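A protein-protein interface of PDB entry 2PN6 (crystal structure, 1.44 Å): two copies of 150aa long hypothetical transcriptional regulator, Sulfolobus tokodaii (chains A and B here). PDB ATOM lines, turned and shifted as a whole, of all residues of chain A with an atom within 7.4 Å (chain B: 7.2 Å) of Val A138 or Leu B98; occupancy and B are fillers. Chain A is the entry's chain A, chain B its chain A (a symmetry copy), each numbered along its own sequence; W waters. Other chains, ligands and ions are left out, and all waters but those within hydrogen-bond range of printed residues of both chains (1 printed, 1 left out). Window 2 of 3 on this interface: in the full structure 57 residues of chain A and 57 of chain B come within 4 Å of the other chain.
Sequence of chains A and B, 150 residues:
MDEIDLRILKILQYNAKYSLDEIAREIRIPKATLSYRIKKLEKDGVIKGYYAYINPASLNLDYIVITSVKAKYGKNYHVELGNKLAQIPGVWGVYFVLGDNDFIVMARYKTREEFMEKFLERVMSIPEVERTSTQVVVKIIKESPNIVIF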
ATOM      1  N   ASP A  62     -24.301  24.018  16.045  1.00  0.00           N
ATOM      2  CA  ASP A  62     -24.327  22.563  16.113  1.00  0.00           C
ATOM      3  C   ASP A  62     -23.979  21.991  17.484  1.00  0.00           C
ATOM      4  O   ASP A  62     -24.163  20.793  17.726  1.00  0.00           O
ATOM      5  CB  ASP A  62     -23.366  22.012  15.051  1.00  0.00           C
ATOM      6  CG  ASP A  62     -23.652  20.570  14.689  1.00  0.00           C
ATOM      7  OD1 ASP A  62     -23.235  19.664  15.440  1.00  0.00           O
ATOM      8  OD2 ASP A  62     -24.304  20.344  13.647  1.00  0.00           O
ATOM      9  N   ILE A  64     -25.176  21.918  20.857  1.00  0.00           N
ATOM     10  CA  ILE A  64     -26.356  22.164  21.670  1.00  0.00           C
ATOM     11  C   ILE A  64     -26.252  21.439  23.002  1.00  0.00           C
ATOM     12  O   ILE A  64     -26.028  20.228  23.044  1.00  0.00           O
ATOM     13  CB  ILE A  64     -27.592  21.683  20.903  1.00  0.00           C
ATOM     14  CG1 ILE A  64     -27.607  22.326  19.511  1.00  0.00           C
ATOM     15  CG2 ILE A  64     -28.858  22.008  21.674  1.00  0.00           C
ATOM     16  CD1 ILE A  64     -27.621  23.842  19.524  1.00  0.00           C
ATOM     17  N   ILE A  66     -27.593  21.007  27.352  1.00  0.00           N
ATOM     18  CA  ILE A  66     -28.579  21.138  28.418  1.00  0.00           C
ATOM     19  C   ILE A  66     -27.736  20.861  29.659  1.00  0.00           C
ATOM     20  O   ILE A  66     -27.306  19.731  29.895  1.00  0.00           O
ATOM     21  CB  ILE A  66     -29.713  20.098  28.273  1.00  0.00           C
ATOM     22  CG1 ILE A  66     -30.439  20.316  26.942  1.00  0.00           C
ATOM     23  CG2 ILE A  66     -30.695  20.237  29.424  1.00  0.00           C
ATOM     24  CD1 ILE A  66     -31.567  19.329  26.658  1.00  0.00           C
ATOM     25  N   SER A 133     -23.288  19.480  35.283  1.00  0.00           N
ATOM     26  CA  SER A 133     -23.246  18.281  34.463  1.00  0.00           C
ATOM     27  C   SER A 133     -23.925  18.649  33.156  1.00  0.00           C
ATOM     28  O   SER A 133     -25.120  18.950  33.125  1.00  0.00           O
ATOM     29  CB  SER A 133     -23.987  17.135  35.139  1.00  0.00           C
ATOM     30  OG  SER A 133     -23.964  15.982  34.307  1.00  0.00           O
ATOM     31  N   THR A 134     -23.154  18.623  32.077  1.00  0.00           N
ATOM     32  CA  THR A 134     -23.669  18.996  30.775  1.00  0.00           C
ATOM     33  C   THR A 134     -24.065  17.816  29.908  1.00  0.00           C
ATOM     34  O   THR A 134     -23.288  16.873  29.714  1.00  0.00           O
ATOM     35  CB  THR A 134     -22.638  19.841  30.009  1.00  0.00           C
ATOM     36  OG1 THR A 134     -22.388  21.052  30.739  1.00  0.00           O
ATOM     37  CG2 THR A 134     -23.151  20.189  28.617  1.00  0.00           C
ATOM     38  N   GLN A 135     -25.296  17.864  29.416  1.00  0.00           N
ATOM     39  CA  GLN A 135     -25.830  16.834  28.537  1.00  0.00           C
ATOM     40  C   GLN A 135     -25.787  17.379  27.114  1.00  0.00           C
ATOM     41  O   GLN A 135     -26.447  18.369  26.805  1.00  0.00           O
ATOM     42  CB  GLN A 135     -27.277  16.501  28.918  1.00  0.00           C
ATOM     43  CG  GLN A 135     -27.415  15.723  30.213  1.00  0.00           C
ATOM     44  CD  GLN A 135     -28.863  15.506  30.612  1.00  0.00           C
ATOM     45  OE1 GLN A 135     -29.427  16.268  31.392  1.00  0.00           O
ATOM     46  NE2 GLN A 135     -29.476  14.468  30.060  1.00  0.00           N
ATOM     47  N   VAL A 136     -24.994  16.746  26.256  1.00  0.00           N
ATOM     48  CA  VAL A 136     -24.880  17.168  24.874  1.00  0.00           C
ATOM     49  C   VAL A 136     -26.062  16.642  24.080  1.00  0.00           C
ATOM     50  O   VAL A 136     -26.424  15.468  24.186  1.00  0.00           O
ATOM     51  CB  VAL A 136     -23.568  16.649  24.258  1.00  0.00           C
ATOM     52  CG1 VAL A 136     -23.506  17.003  22.786  1.00  0.00           C
ATOM     53  CG2 VAL A 136     -22.383  17.254  24.999  1.00  0.00           C
ATOM     54  N   VAL A 137     -26.680  17.519  23.301  1.00  0.00           N
ATOM     55  CA  VAL A 137     -27.815  17.114  22.484  1.00  0.00           C
ATOM     56  C   VAL A 137     -27.300  16.532  21.169  1.00  0.00           C
ATOM     57  O   VAL A 137     -26.654  17.223  20.379  1.00  0.00           O
ATOM     58  CB  VAL A 137     -28.744  18.305  22.199  1.00  0.00           C
ATOM     59  CG1 VAL A 137     -29.848  17.878  21.241  1.00  0.00           C
ATOM     60  CG2 VAL A 137     -29.343  18.822  23.507  1.00  0.00           C
ATOM     61  N   VAL A 138     -27.576  15.250  20.954  1.00  0.00           N
ATOM     62  CA  VAL A 138     -27.148  14.550  19.746  1.00  0.00           C
ATOM     63  C   VAL A 138     -28.101  14.858  18.603  1.00  0.00           C
ATOM     64  O   VAL A 138     -27.694  14.961  17.446  1.00  0.00           O
ATOM     65  CB  VAL A 138     -27.137  13.017  19.964  1.00  0.00           C
ATOM     66  CG1 VAL A 138     -26.688  12.311  18.692  1.00  0.00           C
ATOM     67  CG2 VAL A 138     -26.233  12.664  21.125  1.00  0.00           C
ATOM     68  N   LYS A 139     -29.376  15.007  18.934  1.00  0.00           N
ATOM     69  CA  LYS A 139     -30.382  15.295  17.931  1.00  0.00           C
ATOM     70  C   LYS A 139     -31.581  15.980  18.560  1.00  0.00           C
ATOM     71  O   LYS A 139     -32.062  15.570  19.616  1.00  0.00           O
ATOM     72  CB  LYS A 139     -30.834  13.996  17.258  1.00  0.00           C
ATOM     73  CG  LYS A 139     -31.842  14.186  16.138  1.00  0.00           C
ATOM     74  CD  LYS A 139     -32.265  12.847  15.552  1.00  0.00           C
ATOM     75  CE  LYS A 139     -33.296  13.027  14.449  1.00  0.00           C
ATOM     76  NZ  LYS A 139     -32.775  13.879  13.343  1.00  0.00           N
ATOM     77  N   ILE A 140     -32.046  17.046  17.921  1.00  0.00           N
ATOM     78  CA  ILE A 140     -33.222  17.750  18.401  1.00  0.00           C
ATOM     79  C   ILE A 140     -34.393  17.112  17.664  1.00  0.00           C
ATOM     80  O   ILE A 140     -34.504  17.228  16.441  1.00  0.00           O
ATOM     81  CB  ILE A 140     -33.172  19.252  18.057  1.00  0.00           C
ATOM     82  CG1 ILE A 140     -31.997  19.916  18.779  1.00  0.00           C
ATOM     83  CG2 ILE A 140     -34.494  19.913  18.432  1.00  0.00           C
ATOM     84  CD1 ILE A 140     -31.825  21.399  18.450  1.00  0.00           C
ATOM     85  N   ILE A 141     -35.249  16.415  18.400  1.00  0.00           N
ATOM     86  CA  ILE A 141     -36.406  15.760  17.807  1.00  0.00           C
ATOM     87  C   ILE A 141     -37.494  16.808  17.606  1.00  0.00           C
ATOM     88  O   ILE A 141     -38.206  16.813  16.597  1.00  0.00           O
ATOM     89  CB  ILE A 141     -36.938  14.639  18.737  1.00  0.00           C
ATOM     90  CG1 ILE A 141     -35.834  13.611  19.002  1.00  0.00           C
ATOM     91  CG2 ILE A 141     -38.160  13.973  18.120  1.00  0.00           C
ATOM     92  CD1 ILE A 141     -35.270  12.959  17.757  1.00  0.00           C
ATOM     93  N   HIS B  78     -34.191   5.548  19.585  1.00  0.00           N
ATOM     94  CA  HIS B  78     -34.206   7.003  19.657  1.00  0.00           C
ATOM     95  C   HIS B  78     -35.241   7.602  18.714  1.00  0.00           C
ATOM     96  O   HIS B  78     -35.889   8.597  19.042  1.00  0.00           O
ATOM     97  CB  HIS B  78     -32.807   7.577  19.379  1.00  0.00           C
ATOM     98  CG  HIS B  78     -32.246   7.223  18.032  1.00  0.00           C
ATOM     99  ND1 HIS B  78     -32.359   5.960  17.492  1.00  0.00           N
ATOM    100  CD2 HIS B  78     -31.524   7.952  17.157  1.00  0.00           C
ATOM    101  CE1 HIS B  78     -31.724   5.931  16.330  1.00  0.00           C
ATOM    102  NE2 HIS B  78     -31.210   7.119  16.101  1.00  0.00           N
ATOM    103  N   TYR B  95     -35.321  16.227  23.181  1.00  0.00           N
ATOM    104  CA  TYR B  95     -33.908  16.171  22.843  1.00  0.00           C
ATOM    105  C   TYR B  95     -33.293  14.815  23.140  1.00  0.00           C
ATOM    106  O   TYR B  95     -33.452  14.288  24.243  1.00  0.00           O
ATOM    107  CB  TYR B  95     -33.159  17.223  23.661  1.00  0.00           C
ATOM    108  CG  TYR B  95     -33.705  18.624  23.526  1.00  0.00           C
ATOM    109  CD1 TYR B  95     -33.256  19.468  22.515  1.00  0.00           C
ATOM    110  CD2 TYR B  95     -34.666  19.109  24.416  1.00  0.00           C
ATOM    111  CE1 TYR B  95     -33.742  20.764  22.393  1.00  0.00           C
ATOM    112  CE2 TYR B  95     -35.164  20.401  24.304  1.00  0.00           C
ATOM    113  CZ  TYR B  95     -34.693  21.226  23.293  1.00  0.00           C
ATOM    114  OH  TYR B  95     -35.155  22.516  23.193  1.00  0.00           O
ATOM    115  N   PHE B  96     -32.589  14.255  22.161  1.00  0.00           N
ATOM    116  CA  PHE B  96     -31.893  12.979  22.331  1.00  0.00           C
ATOM    117  C   PHE B  96     -30.526  13.399  22.874  1.00  0.00           C
ATOM    118  O   PHE B  96     -29.781  14.129  22.213  1.00  0.00           O
ATOM    119  CB  PHE B  96     -31.781  12.270  20.978  1.00  0.00           C
ATOM    120  CG  PHE B  96     -31.013  10.980  21.021  1.00  0.00           C
ATOM    121  CD1 PHE B  96     -31.249  10.033  22.019  1.00  0.00           C
ATOM    122  CD2 PHE B  96     -30.055  10.704  20.051  1.00  0.00           C
ATOM    123  CE1 PHE B  96     -30.540   8.827  22.043  1.00  0.00           C
ATOM    124  CE2 PHE B  96     -29.342   9.501  20.064  1.00  0.00           C
ATOM    125  CZ  PHE B  96     -29.584   8.564  21.062  1.00  0.00           C
ATOM    126  N   VAL B  97     -30.197  12.933  24.077  1.00  0.00           N
ATOM    127  CA  VAL B  97     -28.971  13.359  24.744  1.00  0.00           C
ATOM    128  C   VAL B  97     -27.959  12.318  25.199  1.00  0.00           C
ATOM    129  O   VAL B  97     -28.261  11.127  25.322  1.00  0.00           O
ATOM    130  CB  VAL B  97     -29.320  14.209  25.998  1.00  0.00           C
ATOM    131  CG1 VAL B  97     -30.054  15.484  25.583  1.00  0.00           C
ATOM    132  CG2 VAL B  97     -30.184  13.394  26.963  1.00  0.00           C
ATOM    133  N   LEU B  98     -26.750  12.806  25.455  1.00  0.00           N
ATOM    134  CA  LEU B  98     -25.666  11.976  25.962  1.00  0.00           C
ATOM    135  C   LEU B  98     -25.658  12.176  27.469  1.00  0.00           C
ATOM    136  O   LEU B  98     -25.869  13.291  27.948  1.00  0.00           O
ATOM    137  CB  LEU B  98     -24.324  12.419  25.374  1.00  0.00           C
ATOM    138  CG  LEU B  98     -24.194  12.307  23.855  1.00  0.00           C
ATOM    139  CD1 LEU B  98     -22.777  12.677  23.425  1.00  0.00           C
ATOM    140  CD2 LEU B  98     -24.525  10.882  23.421  1.00  0.00           C
ATOM    141  N   GLY B  99     -25.420  11.101  28.208  1.00  0.00           N
ATOM    142  CA  GLY B  99     -25.398  11.171  29.657  1.00  0.00           C
ATOM    143  C   GLY B  99     -26.193  10.039  30.279  1.00  0.00           C
ATOM    144  O   GLY B  99     -26.542   9.076  29.592  1.00  0.00           O
ATOM    145  N   ASP B 100     -26.488  10.164  31.571  1.00  0.00           N
ATOM    146  CA  ASP B 100     -27.226   9.143  32.314  1.00  0.00           C
ATOM    147  C   ASP B 100     -28.688   8.988  31.919  1.00  0.00           C
ATOM    148  O   ASP B 100     -29.387   8.123  32.442  1.00  0.00           O
ATOM    149  CB  ASP B 100     -27.142   9.413  33.819  1.00  0.00           C
ATOM    150  CG  ASP B 100     -25.782   9.080  34.398  1.00  0.00           C
ATOM    151  OD1 ASP B 100     -24.881   8.678  33.632  1.00  0.00           O
ATOM    152  OD2 ASP B 100     -25.614   9.219  35.627  1.00  0.00           O
ATOM    153  N   ASN B 101     -29.160   9.855  31.033  1.00  0.00           N
ATOM    154  CA  ASN B 101     -30.524   9.764  30.542  1.00  0.00           C
ATOM    155  C   ASN B 101     -30.431   9.834  29.028  1.00  0.00           C
ATOM    156  O   ASN B 101     -29.391  10.217  28.486  1.00  0.00           O
ATOM    157  CB  ASN B 101     -31.384  10.889  31.123  1.00  0.00           C
ATOM    158  CG  ASN B 101     -31.637  10.704  32.612  1.00  0.00           C
ATOM    159  OD1 ASN B 101     -32.311   9.759  33.023  1.00  0.00           O
ATOM    160  ND2 ASN B 101     -31.082  11.594  33.422  1.00  0.00           N
ATOM    161  N   ASP B 102     -31.502   9.455  28.342  1.00  0.00           N
ATOM    162  CA  ASP B 102     -31.477   9.427  26.888  1.00  0.00           C
ATOM    163  C   ASP B 102     -32.275  10.527  26.208  1.00  0.00           C
ATOM    164  O   ASP B 102     -31.979  10.902  25.074  1.00  0.00           O
ATOM    165  CB  ASP B 102     -31.928   8.044  26.428  1.00  0.00           C
ATOM    166  CG  ASP B 102     -31.184   6.944  27.151  1.00  0.00           C
ATOM    167  OD1 ASP B 102     -29.934   6.931  27.072  1.00  0.00           O
ATOM    168  OD2 ASP B 102     -31.836   6.107  27.815  1.00  0.00           O
ATOM    169  N   PHE B 103     -33.297  11.032  26.886  1.00  0.00           N
ATOM    170  CA  PHE B 103     -34.083  12.127  26.334  1.00  0.00           C
ATOM    171  C   PHE B 103     -34.393  13.148  27.405  1.00  0.00           C
ATOM    172  O   PHE B 103     -34.505  12.812  28.586  1.00  0.00           O
ATOM    173  CB  PHE B 103     -35.429  11.650  25.762  1.00  0.00           C
ATOM    174  CG  PHE B 103     -35.321  10.963  24.435  1.00  0.00           C
ATOM    175  CD1 PHE B 103     -35.158   9.584  24.355  1.00  0.00           C
ATOM    176  CD2 PHE B 103     -35.391  11.697  23.258  1.00  0.00           C
ATOM    177  CE1 PHE B 103     -35.056   8.954  23.106  1.00  0.00           C
ATOM    178  CE2 PHE B 103     -35.290  11.074  22.017  1.00  0.00           C
ATOM    179  CZ  PHE B 103     -35.127   9.705  21.944  1.00  0.00           C
HETATM  180  O   HOH W   1     -29.489  13.399  32.314  1.00  0.00           O
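Water W1 bridges NE2 of Gln A135 (2.5 Å) and ND2 of Asn B101 (2.7 Å).
No position is printed for both chains. Of the 14 pairs that touch across the chains among the printed residues, none has its exchanged pair printed and touching as well.
The backbone carbonyl oxygen (O) of Ile A64 lies within hydrogen-bond range of the backbone NH (N) of Val A137 (2.8 Å). The backbone carbonyl oxygen (O) of Ile A66 is in hydrogen-bond range of the backbone NH (N) of Gln A135, 2.8 Å away. The backbone NH (N) of Val B97 lies within hydrogen-bond range of the backbone carbonyl oxygen (O) of Asp B102 (2.9 Å).
Of chain B, only Phe B96 and Leu B98 come within 4 Å of Val A138. Of the printed residues of chain A, Leu B98 touches Gln A135, Val A136 and Val A138. Of the printed residues of chain B, Ile A66 touches Tyr B95 (3.8 Å). Of the printed residues of chain A, Val B97 touches Gln A135, Val A136 and Val A137. Of the printed residues of chain B, Ile A141 touches Phe B103. Ser A133 touches none of the printed residues of chain B. Gly B99 touches none of the printed residues of chain A. The nearest residue of chain B that does not touch Val A138 is Val B97 (4.4 Å). The nearest printed residue of chain A that does not touch Leu B98 is Thr A134 (4.8 Å). The nearest printed residue of chain A that does not touch Val B97 is Ile A66 (4.3 Å).
Gln A135 touches Val B97. CA of Gln A135 touches O of Leu B98 (3.6 Å). Val A136 touches Val B97 (O to CA, 3.4 Å). Val A137 touches Tyr B95. CA of Val A137 touches O of Phe B96 (3.6 Å). Val A137 touches Val B97. Val A138 touches Leu B98 (CG2 to CD2, 3.4 Å). Lys A139 touches Tyr B95. Ile A140 touches Tyr B95. Ile A141 touches Phe B103 (CG1 to CE2, 3.98 Å).
Of the 10 printed residues of chain B, 5 touch a printed residue of chain A. Hydrophobic or aromatic side chains of chain B within 4 Å of the printed part of chain A: Tyr B95, Phe B96, Val B97, Leu B98 and Phe B103. Of the 12 printed residues of chain A, 8 touch a printed residue of chain B. Hydrophobic or aromatic side chains of chain A that line the printed part of chain B: Ile A66, Val A137, Val A138, Ile A140 and Ile A141. Along chain A the printed residues that touch a printed residue of chain B span positions 66 to 141. Among the printed residues, 14 pairs touch across the chains.
The backbone NH (N) of Leu B98 sits at hydrogen-bond distance from the backbone carbonyl oxygen (O) of Val A136 (3.0 Å). N of Val A138 sits at hydrogen-bond distance from O of Phe B96 (2.8 Å). The backbone carbonyl oxygen of Lys A139 lies within hydrogen-bond range of the backbone NH of Phe B96 (2.9 Å).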
